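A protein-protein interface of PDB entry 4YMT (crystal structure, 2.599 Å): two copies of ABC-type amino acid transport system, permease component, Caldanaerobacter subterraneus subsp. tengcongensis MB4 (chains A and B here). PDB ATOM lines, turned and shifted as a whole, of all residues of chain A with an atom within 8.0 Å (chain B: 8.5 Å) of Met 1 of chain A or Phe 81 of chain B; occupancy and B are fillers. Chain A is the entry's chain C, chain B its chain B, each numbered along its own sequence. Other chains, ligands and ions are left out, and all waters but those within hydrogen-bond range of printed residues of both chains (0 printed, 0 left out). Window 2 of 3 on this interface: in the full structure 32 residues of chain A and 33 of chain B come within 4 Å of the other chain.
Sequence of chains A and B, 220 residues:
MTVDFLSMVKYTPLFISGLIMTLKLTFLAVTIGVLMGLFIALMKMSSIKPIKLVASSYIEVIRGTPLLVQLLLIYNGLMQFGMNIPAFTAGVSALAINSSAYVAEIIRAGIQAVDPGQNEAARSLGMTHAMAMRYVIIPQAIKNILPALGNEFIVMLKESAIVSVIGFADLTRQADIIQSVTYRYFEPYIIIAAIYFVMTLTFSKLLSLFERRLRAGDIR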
ATOM      1  N   MET A   1      17.077  18.077  11.594  1.00  0.00           N
ATOM      2  CA  MET A   1      17.003  16.850  12.368  1.00  0.00           C
ATOM      3  C   MET A   1      15.583  16.300  12.316  1.00  0.00           C
ATOM      4  O   MET A   1      14.853  16.472  11.329  1.00  0.00           O
ATOM      5  CB  MET A   1      17.430  17.075  13.827  1.00  0.00           C
ATOM      6  CG  MET A   1      18.551  18.082  14.027  1.00  0.00           C
ATOM      7  SD  MET A   1      17.939  19.784  13.921  1.00  0.00           S
ATOM      8  CE  MET A   1      19.352  20.764  14.420  1.00  0.00           C
ATOM      9  N   THR A   2      15.215  15.600  13.380  1.00  0.00           N
ATOM     10  CA  THR A   2      13.839  15.200  13.595  1.00  0.00           C
ATOM     11  C   THR A   2      13.372  15.786  14.931  1.00  0.00           C
ATOM     12  O   THR A   2      14.196  16.259  15.726  1.00  0.00           O
ATOM     13  CB  THR A   2      13.694  13.674  13.591  1.00  0.00           C
ATOM     14  OG1 THR A   2      14.579  13.114  14.573  1.00  0.00           O
ATOM     15  CG2 THR A   2      14.046  13.114  12.217  1.00  0.00           C
ATOM     16  N   VAL A   3      12.062  15.748  15.176  1.00  0.00           N
ATOM     17  CA  VAL A   3      11.469  16.422  16.332  1.00  0.00           C
ATOM     18  C   VAL A   3      11.960  15.898  17.680  1.00  0.00           C
ATOM     19  O   VAL A   3      12.197  14.703  17.851  1.00  0.00           O
ATOM     20  CB  VAL A   3       9.925  16.328  16.300  1.00  0.00           C
ATOM     21  CG1 VAL A   3       9.345  17.329  15.310  1.00  0.00           C
ATOM     22  CG2 VAL A   3       9.486  14.903  15.974  1.00  0.00           C
ATOM     23  N   ASP A   4      12.112  16.810  18.635  1.00  0.00           N
ATOM     24  CA  ASP A   4      12.476  16.431  19.993  1.00  0.00           C
ATOM     25  C   ASP A   4      11.975  17.444  21.010  1.00  0.00           C
ATOM     26  O   ASP A   4      12.666  18.413  21.333  1.00  0.00           O
ATOM     27  CB  ASP A   4      13.986  16.274  20.131  1.00  0.00           C
ATOM     28  CG  ASP A   4      14.383  15.711  21.485  1.00  0.00           C
ATOM     29  OD1 ASP A   4      14.945  16.468  22.309  1.00  0.00           O
ATOM     30  OD2 ASP A   4      14.108  14.513  21.730  1.00  0.00           O
ATOM     31  N   THR A 182      19.556  26.078  20.614  1.00  0.00           N
ATOM     32  CA  THR A 182      19.075  24.735  20.313  1.00  0.00           C
ATOM     33  C   THR A 182      19.079  24.483  18.823  1.00  0.00           C
ATOM     34  O   THR A 182      19.108  23.333  18.380  1.00  0.00           O
ATOM     35  CB  THR A 182      17.625  24.498  20.850  1.00  0.00           C
ATOM     36  OG1 THR A 182      17.486  25.051  22.163  1.00  0.00           O
ATOM     37  CG2 THR A 182      17.303  23.012  20.915  1.00  0.00           C
ATOM     38  N   TYR A 183      19.025  25.577  18.065  1.00  0.00           N
ATOM     39  CA  TYR A 183      18.900  25.550  16.607  1.00  0.00           C
ATOM     40  C   TYR A 183      17.536  24.999  16.160  1.00  0.00           C
ATOM     41  O   TYR A 183      17.318  24.731  14.973  1.00  0.00           O
ATOM     42  CB  TYR A 183      20.037  24.727  15.991  1.00  0.00           C
ATOM     43  CG  TYR A 183      21.403  25.242  16.392  1.00  0.00           C
ATOM     44  CD1 TYR A 183      21.918  26.407  15.839  1.00  0.00           C
ATOM     45  CD2 TYR A 183      22.163  24.575  17.349  1.00  0.00           C
ATOM     46  CE1 TYR A 183      23.152  26.885  16.217  1.00  0.00           C
ATOM     47  CE2 TYR A 183      23.399  25.043  17.733  1.00  0.00           C
ATOM     48  CZ  TYR A 183      23.890  26.198  17.163  1.00  0.00           C
ATOM     49  OH  TYR A 183      25.128  26.670  17.542  1.00  0.00           O
ATOM     50  N   ARG A 184      16.621  24.848  17.114  1.00  0.00           N
ATOM     51  CA  ARG A 184      15.273  24.355  16.834  1.00  0.00           C
ATOM     52  C   ARG A 184      14.217  25.466  16.913  1.00  0.00           C
ATOM     53  O   ARG A 184      14.137  26.197  17.906  1.00  0.00           O
ATOM     54  CB  ARG A 184      14.919  23.212  17.789  1.00  0.00           C
ATOM     55  CG  ARG A 184      15.833  21.996  17.678  1.00  0.00           C
ATOM     56  CD  ARG A 184      15.333  20.881  18.572  1.00  0.00           C
ATOM     57  NE  ARG A 184      15.975  19.597  18.321  1.00  0.00           N
ATOM     58  CZ  ARG A 184      15.654  18.791  17.315  1.00  0.00           C
ATOM     59  NH1 ARG A 184      14.720  19.142  16.444  1.00  0.00           N
ATOM     60  NH2 ARG A 184      16.279  17.637  17.166  1.00  0.00           N
ATOM     61  N   TYR A 185      13.433  25.598  15.848  1.00  0.00           N
ATOM     62  CA  TYR A 185      12.378  26.606  15.780  1.00  0.00           C
ATOM     63  C   TYR A 185      10.988  25.985  15.961  1.00  0.00           C
ATOM     64  O   TYR A 185      10.152  26.516  16.668  1.00  0.00           O
ATOM     65  CB  TYR A 185      12.452  27.346  14.440  1.00  0.00           C
ATOM     66  CG  TYR A 185      13.166  28.678  14.469  1.00  0.00           C
ATOM     67  CD1 TYR A 185      12.860  29.623  15.427  1.00  0.00           C
ATOM     68  CD2 TYR A 185      14.151  28.990  13.529  1.00  0.00           C
ATOM     69  CE1 TYR A 185      13.500  30.858  15.454  1.00  0.00           C
ATOM     70  CE2 TYR A 185      14.804  30.215  13.545  1.00  0.00           C
ATOM     71  CZ  TYR A 185      14.473  31.150  14.512  1.00  0.00           C
ATOM     72  OH  TYR A 185      15.111  32.383  14.550  1.00  0.00           O
ATOM     73  N   PHE A 186      10.779  24.843  15.324  1.00  0.00           N
ATOM     74  CA  PHE A 186       9.498  24.146  15.288  1.00  0.00           C
ATOM     75  C   PHE A 186       8.886  23.895  16.669  1.00  0.00           C
ATOM     76  O   PHE A 186       7.834  24.441  17.007  1.00  0.00           O
ATOM     77  CB  PHE A 186       9.691  22.828  14.565  1.00  0.00           C
ATOM     78  CG  PHE A 186       8.426  22.091  14.292  1.00  0.00           C
ATOM     79  CD1 PHE A 186       7.691  22.358  13.148  1.00  0.00           C
ATOM     80  CD2 PHE A 186       7.982  21.104  15.160  1.00  0.00           C
ATOM     81  CE1 PHE A 186       6.532  21.659  12.878  1.00  0.00           C
ATOM     82  CE2 PHE A 186       6.820  20.400  14.901  1.00  0.00           C
ATOM     83  CZ  PHE A 186       6.089  20.680  13.762  1.00  0.00           C
ATOM     84  N   GLU A 187       9.553  23.057  17.456  1.00  0.00           N
ATOM     85  CA  GLU A 187       9.051  22.640  18.765  1.00  0.00           C
ATOM     86  C   GLU A 187       8.725  23.809  19.726  1.00  0.00           C
ATOM     87  O   GLU A 187       7.680  23.785  20.382  1.00  0.00           O
ATOM     88  CB  GLU A 187      10.048  21.660  19.416  1.00  0.00           C
ATOM     89  CG  GLU A 187      11.484  21.740  18.859  1.00  0.00           C
ATOM     90  CD  GLU A 187      11.778  20.783  17.705  1.00  0.00           C
ATOM     91  OE1 GLU A 187      12.195  21.278  16.636  1.00  0.00           O
ATOM     92  OE2 GLU A 187      11.634  19.548  17.873  1.00  0.00           O
ATOM     93  N   LEU B  73       5.896  29.688  12.478  1.00  0.00           N
ATOM     94  CA  LEU B  73       5.914  28.227  12.515  1.00  0.00           C
ATOM     95  C   LEU B  73       6.110  27.641  11.116  1.00  0.00           C
ATOM     96  O   LEU B  73       6.816  26.639  10.951  1.00  0.00           O
ATOM     97  CB  LEU B  73       4.630  27.681  13.137  1.00  0.00           C
ATOM     98  CG  LEU B  73       4.471  26.170  13.299  1.00  0.00           C
ATOM     99  CD1 LEU B  73       5.672  25.565  13.996  1.00  0.00           C
ATOM    100  CD2 LEU B  73       3.205  25.899  14.099  1.00  0.00           C
ATOM    101  N   ILE B  74       5.524  28.276  10.105  1.00  0.00           N
ATOM    102  CA  ILE B  74       5.777  27.812   8.746  1.00  0.00           C
ATOM    103  C   ILE B  74       7.191  28.203   8.269  1.00  0.00           C
ATOM    104  O   ILE B  74       7.923  27.381   7.708  1.00  0.00           O
ATOM    105  CB  ILE B  74       4.738  28.368   7.752  1.00  0.00           C
ATOM    106  CG1 ILE B  74       3.323  27.913   8.133  1.00  0.00           C
ATOM    107  CG2 ILE B  74       5.091  27.951   6.321  1.00  0.00           C
ATOM    108  CD1 ILE B  74       2.295  28.184   7.063  1.00  0.00           C
ATOM    109  N   ASN B  76      10.072  29.623   9.981  1.00  0.00           N
ATOM    110  CA  ASN B  76      11.259  29.276  10.749  1.00  0.00           C
ATOM    111  C   ASN B  76      11.227  27.812  11.167  1.00  0.00           C
ATOM    112  O   ASN B  76      12.224  27.099  11.059  1.00  0.00           O
ATOM    113  CB  ASN B  76      11.374  30.163  11.989  1.00  0.00           C
ATOM    114  CG  ASN B  76      11.636  31.613  11.645  1.00  0.00           C
ATOM    115  OD1 ASN B  76      11.980  31.931  10.508  1.00  0.00           O
ATOM    116  ND2 ASN B  76      11.462  32.504  12.621  1.00  0.00           N
ATOM    117  N   GLY B  77      10.064  27.362  11.623  1.00  0.00           N
ATOM    118  CA  GLY B  77       9.927  26.015  12.128  1.00  0.00           C
ATOM    119  C   GLY B  77      10.244  24.953  11.103  1.00  0.00           C
ATOM    120  O   GLY B  77      10.613  23.837  11.467  1.00  0.00           O
ATOM    121  N   LEU B  78      10.140  25.288   9.822  1.00  0.00           N
ATOM    122  CA  LEU B  78      10.358  24.277   8.796  1.00  0.00           C
ATOM    123  C   LEU B  78      11.796  24.224   8.277  1.00  0.00           C
ATOM    124  O   LEU B  78      12.159  23.303   7.528  1.00  0.00           O
ATOM    125  CB  LEU B  78       9.390  24.500   7.635  1.00  0.00           C
ATOM    126  CG  LEU B  78       7.947  24.221   8.061  1.00  0.00           C
ATOM    127  CD1 LEU B  78       6.989  24.301   6.878  1.00  0.00           C
ATOM    128  CD2 LEU B  78       7.854  22.873   8.770  1.00  0.00           C
ATOM    129  N   MET B  79      12.617  25.191   8.690  1.00  0.00           N
ATOM    130  CA  MET B  79      14.006  25.248   8.233  1.00  0.00           C
ATOM    131  C   MET B  79      14.785  24.008   8.667  1.00  0.00           C
ATOM    132  O   MET B  79      15.418  23.340   7.844  1.00  0.00           O
ATOM    133  CB  MET B  79      14.676  26.522   8.738  1.00  0.00           C
ATOM    134  CG  MET B  79      14.441  27.708   7.813  1.00  0.00           C
ATOM    135  SD  MET B  79      14.812  29.291   8.596  1.00  0.00           S
ATOM    136  CE  MET B  79      14.239  30.437   7.336  1.00  0.00           C
ATOM    137  N   GLN B  80      14.676  23.662   9.947  1.00  0.00           N
ATOM    138  CA  GLN B  80      15.381  22.510  10.501  1.00  0.00           C
ATOM    139  C   GLN B  80      14.941  21.180   9.906  1.00  0.00           C
ATOM    140  O   GLN B  80      15.241  20.129  10.461  1.00  0.00           O
ATOM    141  CB  GLN B  80      15.189  22.458  12.010  1.00  0.00           C
ATOM    142  CG  GLN B  80      13.735  22.404  12.421  1.00  0.00           C
ATOM    143  CD  GLN B  80      13.548  22.673  13.893  1.00  0.00           C
ATOM    144  OE1 GLN B  80      13.431  23.828  14.315  1.00  0.00           O
ATOM    145  NE2 GLN B  80      13.540  21.608  14.691  1.00  0.00           N
ATOM    146  N   PHE B  81      14.217  21.216   8.795  1.00  0.00           N
ATOM    147  CA  PHE B  81      13.831  19.989   8.120  1.00  0.00           C
ATOM    148  C   PHE B  81      14.411  19.988   6.713  1.00  0.00           C
ATOM    149  O   PHE B  81      14.099  19.118   5.897  1.00  0.00           O
ATOM    150  CB  PHE B  81      12.309  19.853   8.066  1.00  0.00           C
ATOM    151  CG  PHE B  81      11.663  19.713   9.414  1.00  0.00           C
ATOM    152  CD1 PHE B  81      11.889  18.589  10.194  1.00  0.00           C
ATOM    153  CD2 PHE B  81      10.821  20.701   9.901  1.00  0.00           C
ATOM    154  CE1 PHE B  81      11.293  18.452  11.440  1.00  0.00           C
ATOM    155  CE2 PHE B  81      10.221  20.572  11.147  1.00  0.00           C
ATOM    156  CZ  PHE B  81      10.457  19.444  11.917  1.00  0.00           C
ATOM    157  N   GLY B  82      15.290  20.945   6.441  1.00  0.00           N
ATOM    158  CA  GLY B  82      15.860  21.071   5.112  1.00  0.00           C
ATOM    159  C   GLY B  82      14.828  21.637   4.157  1.00  0.00           C
ATOM    160  O   GLY B  82      14.912  21.475   2.934  1.00  0.00           O
ATOM    161  N   MET B  83      13.839  22.299   4.745  1.00  0.00           N
ATOM    162  CA  MET B  83      12.770  22.941   4.003  1.00  0.00           C
ATOM    163  C   MET B  83      12.946  24.449   4.133  1.00  0.00           C
ATOM    164  O   MET B  83      12.764  25.018   5.212  1.00  0.00           O
ATOM    165  CB  MET B  83      11.401  22.493   4.531  1.00  0.00           C
ATOM    166  CG  MET B  83      10.225  22.727   3.583  1.00  0.00           C
ATOM    167  SD  MET B  83      10.389  21.903   1.980  1.00  0.00           S
ATOM    168  CE  MET B  83       8.909  22.458   1.120  1.00  0.00           C
ATOM    169  N   ASN B  84      13.366  25.087   3.048  1.00  0.00           N
ATOM    170  CA  ASN B  84      13.479  26.535   3.044  1.00  0.00           C
ATOM    171  C   ASN B  84      12.464  27.157   2.104  1.00  0.00           C
ATOM    172  O   ASN B  84      12.774  27.401   0.937  1.00  0.00           O
ATOM    173  CB  ASN B  84      14.878  26.982   2.645  1.00  0.00           C
ATOM    174  CG  ASN B  84      15.064  28.480   2.804  1.00  0.00           C
ATOM    175  OD1 ASN B  84      15.494  28.954   3.861  1.00  0.00           O
ATOM    176  ND2 ASN B  84      14.714  29.236   1.766  1.00  0.00           N
ATOM    177  N   ILE B  85      11.261  27.424   2.610  1.00  0.00           N
ATOM    178  CA  ILE B  85      10.216  28.033   1.799  1.00  0.00           C
ATOM    179  C   ILE B  85      10.436  29.543   1.720  1.00  0.00           C
ATOM    180  O   ILE B  85      10.808  30.177   2.716  1.00  0.00           O
ATOM    181  CB  ILE B  85       8.777  27.717   2.347  1.00  0.00           C
ATOM    182  CG1 ILE B  85       8.670  27.942   3.863  1.00  0.00           C
ATOM    183  CG2 ILE B  85       8.387  26.278   2.014  1.00  0.00           C
ATOM    184  CD1 ILE B  85       8.917  26.675   4.708  1.00  0.00           C
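N of Met 1 of chain A sits at hydrogen-bond distance from O of Gln 80 of chain B, 3.0 Å away. The guanidinium group of Arg 184 of chain A sits close to the side-chain amide nitrogen of Gln 80 of chain B. N of Phe 186 of chain A sits at hydrogen-bond distance from OE1 of Gln 80 of chain B, at 3.0 Å. The backbone NH (N) of Tyr 185 of chain A sits close to the side-chain amide oxygen (OE1) of Gln 80 of chain B, 2.3 Å away. The side-chain carboxylate of Glu 187 of chain A sits close to the side-chain amide nitrogen of Gln 80 of chain B.
O of Thr 2 of chain A sits at hydrogen-bond distance from NH2 of Arg 184 of chain A (2.9 Å). N of Asp 4 of chain A is in hydrogen-bond range of OE2 of Glu 187 of chain A, 2.9 Å away. NH1 of Arg 184 of chain A is in salt-bridge range of OE1 of Glu 187 of chain A, at 3.3 Å.
Phe 81 of chain B touches Met 1 of chain A (CD1 to O, 3.8 Å). Tyr 185 of chain A touches Asn 76 of chain B. Tyr 185 of chain A touches Gly 77 of chain B. CD1 of Leu 73 of chain B touches O of Phe 186 of chain A, at 3.9 Å. Phe 186 of chain A touches Gly 77 of chain B (CB to O, 3.4 Å). Phe 81 of chain B touches Phe 186 of chain A.
Of chain B, only Gln 80 and Phe 81 come within 4 Å of Met 1 of chain A. Phe 81 of chain B touches two residues of chain A. Of the printed residues of chain A, Gly 77 of chain B touches Tyr 185 (3.7 Å) and Phe 186 (3.4 Å). Of the printed residues of chain A, Leu 73 of chain B touches Phe 186 (3.9 Å). Printed residues of chain B within 4 Å of Phe 186 of chain A: Leu 73 (3.9 Å), Gly 77 (3.4 Å), Gln 80 (3.0 Å) and Phe 81 (3.7 Å). Of the printed residues of chain A, Gln 80 of chain B touches Met 1, Arg 184, Tyr 185, Phe 186 and Glu 187. Thr 182 of chain A touches none of the printed residues of chain B.
Printed residues of chain B that touch a printed residue of chain A: Leu 73, Asn 76, Gly 77, Gln 80 and Phe 81. Hydrophobic or aromatic side chains of chain B within 4 Å of the printed part of chain A: Leu 73 and Phe 81. Of the 10 printed residues of chain A, 5 touch a printed residue of chain B. Among the printed residues, 11 pairs touch across the chains. Among the printed residues, no Asp or Glu carboxylate lies within 4 Å of a Lys or Arg side-chain nitrogen of the other chain.
No position is printed for both chains. Of the 11 pairs that touch across the chains among the printed residues, none has its exchanged pair printed and touching as well.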
